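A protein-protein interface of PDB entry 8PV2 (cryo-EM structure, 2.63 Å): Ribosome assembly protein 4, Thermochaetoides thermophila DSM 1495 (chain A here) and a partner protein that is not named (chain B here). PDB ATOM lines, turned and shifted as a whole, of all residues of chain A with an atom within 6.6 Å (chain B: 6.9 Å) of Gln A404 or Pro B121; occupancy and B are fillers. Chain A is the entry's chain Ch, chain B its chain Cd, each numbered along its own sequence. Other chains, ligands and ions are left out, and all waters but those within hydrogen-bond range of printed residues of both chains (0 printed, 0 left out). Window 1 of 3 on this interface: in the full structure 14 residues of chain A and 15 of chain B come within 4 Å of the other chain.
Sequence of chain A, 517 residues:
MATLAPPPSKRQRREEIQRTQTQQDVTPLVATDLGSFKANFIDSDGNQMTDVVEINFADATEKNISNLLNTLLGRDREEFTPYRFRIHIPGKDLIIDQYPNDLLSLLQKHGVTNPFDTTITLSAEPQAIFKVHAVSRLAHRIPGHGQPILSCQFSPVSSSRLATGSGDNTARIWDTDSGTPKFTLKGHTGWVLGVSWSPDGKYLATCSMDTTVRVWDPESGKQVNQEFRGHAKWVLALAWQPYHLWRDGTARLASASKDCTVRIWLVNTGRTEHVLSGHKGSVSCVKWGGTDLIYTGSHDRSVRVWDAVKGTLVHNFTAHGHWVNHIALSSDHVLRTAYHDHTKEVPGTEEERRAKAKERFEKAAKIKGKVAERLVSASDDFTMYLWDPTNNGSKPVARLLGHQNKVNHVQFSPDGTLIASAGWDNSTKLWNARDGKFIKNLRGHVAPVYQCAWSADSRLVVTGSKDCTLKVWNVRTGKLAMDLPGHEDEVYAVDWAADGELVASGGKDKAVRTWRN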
ATOM      1  N   PHE A 382       4.549 -20.921 -13.072  1.00  0.00           N
ATOM      2  CA  PHE A 382       3.120 -20.660 -13.242  1.00  0.00           C
ATOM      3  C   PHE A 382       2.347 -21.945 -13.492  1.00  0.00           C
ATOM      4  O   PHE A 382       1.147 -21.893 -13.764  1.00  0.00           O
ATOM      5  CB  PHE A 382       2.783 -19.675 -14.378  1.00  0.00           C
ATOM      6  CG  PHE A 382       3.419 -18.300 -14.270  1.00  0.00           C
ATOM      7  CD1 PHE A 382       4.184 -17.910 -13.181  1.00  0.00           C
ATOM      8  CD2 PHE A 382       3.215 -17.383 -15.279  1.00  0.00           C
ATOM      9  CE1 PHE A 382       4.745 -16.660 -13.122  1.00  0.00           C
ATOM     10  CE2 PHE A 382       3.769 -16.131 -15.218  1.00  0.00           C
ATOM     11  CZ  PHE A 382       4.532 -15.768 -14.137  1.00  0.00           C
ATOM     12  N   GLY A 402      -2.528 -22.603 -16.865  1.00  0.00           N
ATOM     13  CA  GLY A 402      -3.654 -21.714 -16.666  1.00  0.00           C
ATOM     14  C   GLY A 402      -3.476 -20.599 -15.662  1.00  0.00           C
ATOM     15  O   GLY A 402      -4.153 -19.574 -15.767  1.00  0.00           O
ATOM     16  N   HIS A 403      -2.585 -20.764 -14.694  1.00  0.00           N
ATOM     17  CA  HIS A 403      -2.284 -19.665 -13.789  1.00  0.00           C
ATOM     18  C   HIS A 403      -1.426 -18.619 -14.485  1.00  0.00           C
ATOM     19  O   HIS A 403      -0.530 -18.944 -15.266  1.00  0.00           O
ATOM     20  CB  HIS A 403      -1.584 -20.179 -12.537  1.00  0.00           C
ATOM     21  CG  HIS A 403      -2.517 -20.752 -11.520  1.00  0.00           C
ATOM     22  ND1 HIS A 403      -3.290 -19.962 -10.699  1.00  0.00           N
ATOM     23  CD2 HIS A 403      -2.812 -22.031 -11.197  1.00  0.00           C
ATOM     24  CE1 HIS A 403      -4.019 -20.729  -9.911  1.00  0.00           C
ATOM     25  NE2 HIS A 403      -3.745 -21.990 -10.191  1.00  0.00           N
ATOM     26  N   GLN A 404      -1.717 -17.351 -14.206  1.00  0.00           N
ATOM     27  CA  GLN A 404      -1.003 -16.227 -14.792  1.00  0.00           C
ATOM     28  C   GLN A 404       0.105 -15.710 -13.886  1.00  0.00           C
ATOM     29  O   GLN A 404       0.771 -14.730 -14.228  1.00  0.00           O
ATOM     30  CB  GLN A 404      -1.978 -15.101 -15.125  1.00  0.00           C
ATOM     31  CG  GLN A 404      -3.235 -15.554 -15.846  1.00  0.00           C
ATOM     32  CD  GLN A 404      -2.997 -15.832 -17.309  1.00  0.00           C
ATOM     33  OE1 GLN A 404      -2.902 -16.982 -17.727  1.00  0.00           O
ATOM     34  NE2 GLN A 404      -2.895 -14.776 -18.100  1.00  0.00           N
ATOM     35  N   ASN A 405       0.308 -16.341 -12.739  1.00  0.00           N
ATOM     36  CA  ASN A 405       1.373 -15.963 -11.825  1.00  0.00           C
ATOM     37  C   ASN A 405       1.773 -17.209 -11.052  1.00  0.00           C
ATOM     38  O   ASN A 405       1.275 -18.305 -11.322  1.00  0.00           O
ATOM     39  CB  ASN A 405       0.933 -14.830 -10.900  1.00  0.00           C
ATOM     40  CG  ASN A 405       2.075 -13.935 -10.488  1.00  0.00           C
ATOM     41  OD1 ASN A 405       3.228 -14.345 -10.469  1.00  0.00           O
ATOM     42  ND2 ASN A 405       1.754 -12.697 -10.156  1.00  0.00           N
ATOM     43  N   LYS A 406       2.690 -17.032 -10.100  1.00  0.00           N
ATOM     44  CA  LYS A 406       3.257 -18.151  -9.355  1.00  0.00           C
ATOM     45  C   LYS A 406       2.179 -18.895  -8.584  1.00  0.00           C
ATOM     46  O   LYS A 406       1.219 -18.298  -8.093  1.00  0.00           O
ATOM     47  CB  LYS A 406       4.332 -17.660  -8.384  1.00  0.00           C
ATOM     48  CG  LYS A 406       5.418 -16.815  -9.008  1.00  0.00           C
ATOM     49  CD  LYS A 406       6.413 -16.334  -7.972  1.00  0.00           C
ATOM     50  CE  LYS A 406       5.798 -15.313  -7.050  1.00  0.00           C
ATOM     51  NZ  LYS A 406       5.417 -14.078  -7.781  1.00  0.00           N
ATOM     52  N   TRP A 424      -0.774 -16.740  -7.197  1.00  0.00           N
ATOM     53  CA  TRP A 424      -0.474 -15.340  -6.945  1.00  0.00           C
ATOM     54  C   TRP A 424      -1.180 -14.413  -7.916  1.00  0.00           C
ATOM     55  O   TRP A 424      -1.016 -13.194  -7.824  1.00  0.00           O
ATOM     56  CB  TRP A 424       1.034 -15.099  -7.007  1.00  0.00           C
ATOM     57  CG  TRP A 424       1.798 -15.643  -5.848  1.00  0.00           C
ATOM     58  CD1 TRP A 424       1.771 -16.917  -5.369  1.00  0.00           C
ATOM     59  CD2 TRP A 424       2.731 -14.930  -5.033  1.00  0.00           C
ATOM     60  NE1 TRP A 424       2.620 -17.041  -4.300  1.00  0.00           N
ATOM     61  CE2 TRP A 424       3.221 -15.832  -4.074  1.00  0.00           C
ATOM     62  CE3 TRP A 424       3.192 -13.614  -5.017  1.00  0.00           C
ATOM     63  CZ2 TRP A 424       4.149 -15.461  -3.113  1.00  0.00           C
ATOM     64  CZ3 TRP A 424       4.111 -13.249  -4.063  1.00  0.00           C
ATOM     65  CH2 TRP A 424       4.581 -14.168  -3.126  1.00  0.00           C
ATOM     66  N   ASP A 425      -1.956 -14.963  -8.847  1.00  0.00           N
ATOM     67  CA  ASP A 425      -2.797 -14.183  -9.737  1.00  0.00           C
ATOM     68  C   ASP A 425      -4.206 -14.014  -9.184  1.00  0.00           C
ATOM     69  O   ASP A 425      -5.165 -13.937  -9.958  1.00  0.00           O
ATOM     70  CB  ASP A 425      -2.842 -14.829 -11.119  1.00  0.00           C
ATOM     71  CG  ASP A 425      -3.175 -16.301 -11.061  1.00  0.00           C
ATOM     72  OD1 ASP A 425      -3.171 -16.871  -9.957  1.00  0.00           O
ATOM     73  OD2 ASP A 425      -3.457 -16.885 -12.124  1.00  0.00           O
ATOM     74  N   SER A 427      -6.241 -16.016  -7.751  1.00  0.00           N
ATOM     75  CA  SER A 427      -7.232 -16.992  -8.170  1.00  0.00           C
ATOM     76  C   SER A 427      -6.938 -18.378  -7.616  1.00  0.00           C
ATOM     77  O   SER A 427      -5.790 -18.761  -7.364  1.00  0.00           O
ATOM     78  CB  SER A 427      -7.328 -17.075  -9.695  1.00  0.00           C
ATOM     79  OG  SER A 427      -6.249 -17.821 -10.222  1.00  0.00           O
ATOM     80  N   LYS A 429      -7.905 -22.334  -8.748  1.00  0.00           N
ATOM     81  CA  LYS A 429      -8.331 -23.086  -9.919  1.00  0.00           C
ATOM     82  C   LYS A 429      -8.569 -24.544  -9.565  1.00  0.00           C
ATOM     83  O   LYS A 429      -7.915 -25.096  -8.674  1.00  0.00           O
ATOM     84  CB  LYS A 429      -7.315 -22.987 -11.053  1.00  0.00           C
ATOM     85  CG  LYS A 429      -7.324 -21.655 -11.759  1.00  0.00           C
ATOM     86  CD  LYS A 429      -6.373 -21.649 -12.926  1.00  0.00           C
ATOM     87  CE  LYS A 429      -6.690 -20.506 -13.853  1.00  0.00           C
ATOM     88  NZ  LYS A 429      -6.516 -19.200 -13.176  1.00  0.00           N
ATOM     89  N   ARG B 118     -13.251  -7.099 -16.037  1.00  0.00           N
ATOM     90  CA  ARG B 118     -12.874  -7.683 -17.315  1.00  0.00           C
ATOM     91  C   ARG B 118     -12.118  -8.987 -17.096  1.00  0.00           C
ATOM     92  O   ARG B 118     -11.523  -9.217 -16.039  1.00  0.00           O
ATOM     93  CB  ARG B 118     -12.015  -6.719 -18.130  1.00  0.00           C
ATOM     94  CG  ARG B 118     -10.649  -6.455 -17.535  1.00  0.00           C
ATOM     95  CD  ARG B 118      -9.811  -5.571 -18.434  1.00  0.00           C
ATOM     96  NE  ARG B 118     -10.370  -4.235 -18.589  1.00  0.00           N
ATOM     97  CZ  ARG B 118      -9.736  -3.118 -18.258  1.00  0.00           C
ATOM     98  NH1 ARG B 118      -8.530  -3.143 -17.716  1.00  0.00           N
ATOM     99  NH2 ARG B 118     -10.328  -1.948 -18.475  1.00  0.00           N
ATOM    100  N   ASP B 119     -12.159  -9.852 -18.103  1.00  0.00           N
ATOM    101  CA  ASP B 119     -11.478 -11.133 -18.009  1.00  0.00           C
ATOM    102  C   ASP B 119      -9.961 -10.964 -18.069  1.00  0.00           C
ATOM    103  O   ASP B 119      -9.434  -9.951 -18.534  1.00  0.00           O
ATOM    104  CB  ASP B 119     -12.045 -12.106 -19.062  1.00  0.00           C
ATOM    105  CG  ASP B 119     -11.539 -11.879 -20.513  1.00  0.00           C
ATOM    106  OD1 ASP B 119     -10.644 -11.064 -20.834  1.00  0.00           O
ATOM    107  OD2 ASP B 119     -12.088 -12.579 -21.388  1.00  0.00           O
ATOM    108  N   GLY B 120      -9.258 -11.972 -17.569  1.00  0.00           N
ATOM    109  CA  GLY B 120      -7.815 -11.953 -17.569  1.00  0.00           C
ATOM    110  C   GLY B 120      -7.249 -12.190 -18.949  1.00  0.00           C
ATOM    111  O   GLY B 120      -7.948 -12.600 -19.889  1.00  0.00           O
ATOM    112  N   PRO B 121      -5.957 -11.900 -19.097  1.00  0.00           N
ATOM    113  CA  PRO B 121      -5.261 -12.224 -20.345  1.00  0.00           C
ATOM    114  C   PRO B 121      -5.287 -13.716 -20.645  1.00  0.00           C
ATOM    115  O   PRO B 121      -5.577 -14.555 -19.789  1.00  0.00           O
ATOM    116  CB  PRO B 121      -3.825 -11.754 -20.081  1.00  0.00           C
ATOM    117  CG  PRO B 121      -3.883 -10.913 -18.809  1.00  0.00           C
ATOM    118  CD  PRO B 121      -5.314 -10.765 -18.416  1.00  0.00           C
ATOM    119  N   LYS B 122      -4.970 -14.040 -21.895  1.00  0.00           N
ATOM    120  CA  LYS B 122      -4.963 -15.430 -22.323  1.00  0.00           C
ATOM    121  C   LYS B 122      -3.787 -16.178 -21.704  1.00  0.00           C
ATOM    122  O   LYS B 122      -2.826 -15.578 -21.216  1.00  0.00           O
ATOM    123  CB  LYS B 122      -4.902 -15.516 -23.848  1.00  0.00           C
ATOM    124  CG  LYS B 122      -6.069 -14.865 -24.616  1.00  0.00           C
ATOM    125  CD  LYS B 122      -7.418 -15.604 -24.507  1.00  0.00           C
ATOM    126  CE  LYS B 122      -8.336 -15.088 -23.394  1.00  0.00           C
ATOM    127  NZ  LYS B 122      -9.662 -15.768 -23.408  1.00  0.00           N
ATOM    128  N   LEU B 123      -3.885 -17.511 -21.733  1.00  0.00           N
ATOM    129  CA  LEU B 123      -2.888 -18.371 -21.099  1.00  0.00           C
ATOM    130  C   LEU B 123      -1.516 -18.212 -21.748  1.00  0.00           C
ATOM    131  O   LEU B 123      -0.506 -18.019 -21.053  1.00  0.00           O
ATOM    132  CB  LEU B 123      -3.362 -19.825 -21.191  1.00  0.00           C
ATOM    133  CG  LEU B 123      -2.690 -21.013 -20.504  1.00  0.00           C
ATOM    134  CD1 LEU B 123      -3.744 -22.080 -20.280  1.00  0.00           C
ATOM    135  CD2 LEU B 123      -1.534 -21.596 -21.305  1.00  0.00           C
ATOM    136  N   GLU B 124      -1.464 -18.295 -23.080  1.00  0.00           N
ATOM    137  CA  GLU B 124      -0.190 -18.224 -23.783  1.00  0.00           C
ATOM    138  C   GLU B 124       0.427 -16.837 -23.659  1.00  0.00           C
ATOM    139  O   GLU B 124       1.651 -16.701 -23.557  1.00  0.00           O
ATOM    140  CB  GLU B 124      -0.374 -18.634 -25.252  1.00  0.00           C
ATOM    141  CG  GLU B 124      -1.195 -17.684 -26.125  1.00  0.00           C
ATOM    142  CD  GLU B 124      -2.692 -17.933 -26.043  1.00  0.00           C
ATOM    143  OE1 GLU B 124      -3.141 -18.629 -25.109  1.00  0.00           O
ATOM    144  OE2 GLU B 124      -3.423 -17.426 -26.920  1.00  0.00           O
ATOM    145  N   ASP B 125      -0.411 -15.796 -23.632  1.00  0.00           N
ATOM    146  CA  ASP B 125       0.096 -14.446 -23.413  1.00  0.00           C
ATOM    147  C   ASP B 125       0.672 -14.297 -22.013  1.00  0.00           C
ATOM    148  O   ASP B 125       1.758 -13.734 -21.840  1.00  0.00           O
ATOM    149  CB  ASP B 125      -1.012 -13.422 -23.653  1.00  0.00           C
ATOM    150  CG  ASP B 125      -1.413 -13.330 -25.109  1.00  0.00           C
ATOM    151  OD1 ASP B 125      -0.554 -13.586 -25.979  1.00  0.00           O
ATOM    152  OD2 ASP B 125      -2.585 -13.000 -25.387  1.00  0.00           O
ATOM    153  N   GLY B 126      -0.030 -14.822 -21.004  1.00  0.00           N
ATOM    154  CA  GLY B 126       0.460 -14.723 -19.638  1.00  0.00           C
ATOM    155  C   GLY B 126       1.762 -15.470 -19.426  1.00  0.00           C
ATOM    156  O   GLY B 126       2.597 -15.062 -18.617  1.00  0.00           O
ATOM    157  N   LEU B 127       1.949 -16.578 -20.145  1.00  0.00           N
ATOM    158  CA  LEU B 127       3.234 -17.268 -20.070  1.00  0.00           C
ATOM    159  C   LEU B 127       4.332 -16.531 -20.832  1.00  0.00           C
ATOM    160  O   LEU B 127       5.464 -16.423 -20.340  1.00  0.00           O
ATOM    161  CB  LEU B 127       3.099 -18.698 -20.585  1.00  0.00           C
ATOM    162  CG  LEU B 127       2.218 -19.613 -19.741  1.00  0.00           C
ATOM    163  CD1 LEU B 127       2.044 -20.959 -20.419  1.00  0.00           C
ATOM    164  CD2 LEU B 127       2.826 -19.781 -18.363  1.00  0.00           C
ATOM    165  N   HIS B 130       6.272 -13.485 -19.408  1.00  0.00           N
ATOM    166  CA  HIS B 130       7.191 -13.734 -18.313  1.00  0.00           C
ATOM    167  C   HIS B 130       8.239 -14.786 -18.625  1.00  0.00           C
ATOM    168  O   HIS B 130       9.070 -15.068 -17.754  1.00  0.00           O
ATOM    169  CB  HIS B 130       6.410 -14.142 -17.060  1.00  0.00           C
ATOM    170  CG  HIS B 130       5.344 -13.166 -16.681  1.00  0.00           C
ATOM    171  ND1 HIS B 130       4.012 -13.367 -16.971  1.00  0.00           N
ATOM    172  CD2 HIS B 130       5.413 -11.975 -16.042  1.00  0.00           C
ATOM    173  CE1 HIS B 130       3.306 -12.344 -16.524  1.00  0.00           C
ATOM    174  NE2 HIS B 130       4.133 -11.485 -15.955  1.00  0.00           N
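The backbone carbonyl oxygen (O) of Gly B126 is in hydrogen-bond range of a ring nitrogen (ND1) of His B130 (2.8 Å).
The backbone carbonyl oxygen (O) of Gly A402 lies close to the side-chain amide oxygen (OE1) of Gln A404 (3.5 Å).
OD2 of Asp A425 is in hydrogen-bond range of N of Gln A404 (2.8 Å).
Among the printed residues, pairs that only touch across the chains: Phe A382 with Gly B126 (3.8 Å), Phe A382 with Leu B127 (3.9 Å), Phe A382 with His B130 (3.3 Å), Gly A402 with Leu B123 (3.6 Å), Gln A404 with Leu B123 (3.6 Å) and Gln A404 with Gly B126 (3.7 Å).
Of the 10 printed residues of chain A, 3 touch a printed residue of chain B.
Hydrophobic or aromatic side chains of chain A within 4 Å of the printed part of chain B: Phe A382.
Of the 11 printed residues of chain B, 6 touch a printed residue of chain A.
Among the printed residues, no Asp or Glu carboxylate lies within 4 Å of a Lys or Arg side-chain nitrogen of the other chain.
Printed residues of chain B within 4 Å of Gln A404: Pro B121 (3.2 Å), Lys B122 (3.2 Å), Leu B123 (3.6 Å) and Gly B126 (3.7 Å).
Of chain A, only Gln A404 comes within 4 Å of Pro B121.
Printed residues of chain A within 4 Å of His B130: Phe A382.
Printed residues of chain B within 4 Å of Gly A402: Leu B123.
Of the printed residues of chain A, Leu B123 touches Gly A402 and Gln A404.
Of the printed residues of chain B, Phe A382 touches Gly B126, Leu B127 and His B130.
Of the printed residues of chain A, Gly B126 touches Phe A382 and Gln A404.
Ser A427 touches none of the printed residues of chain B.
Asp B119 touches none of the printed residues of chain A.
The nearest printed residue of chain A that does not touch Pro B121 is Gly A402 (6.6 Å).
O of Pro B121 lies within hydrogen-bond range of NE2 of Gln A404.
The side-chain amide nitrogen (NE2) of Gln A404 is in hydrogen-bond range of the backbone carbonyl oxygen (O) of Lys B122 (3.2 Å).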
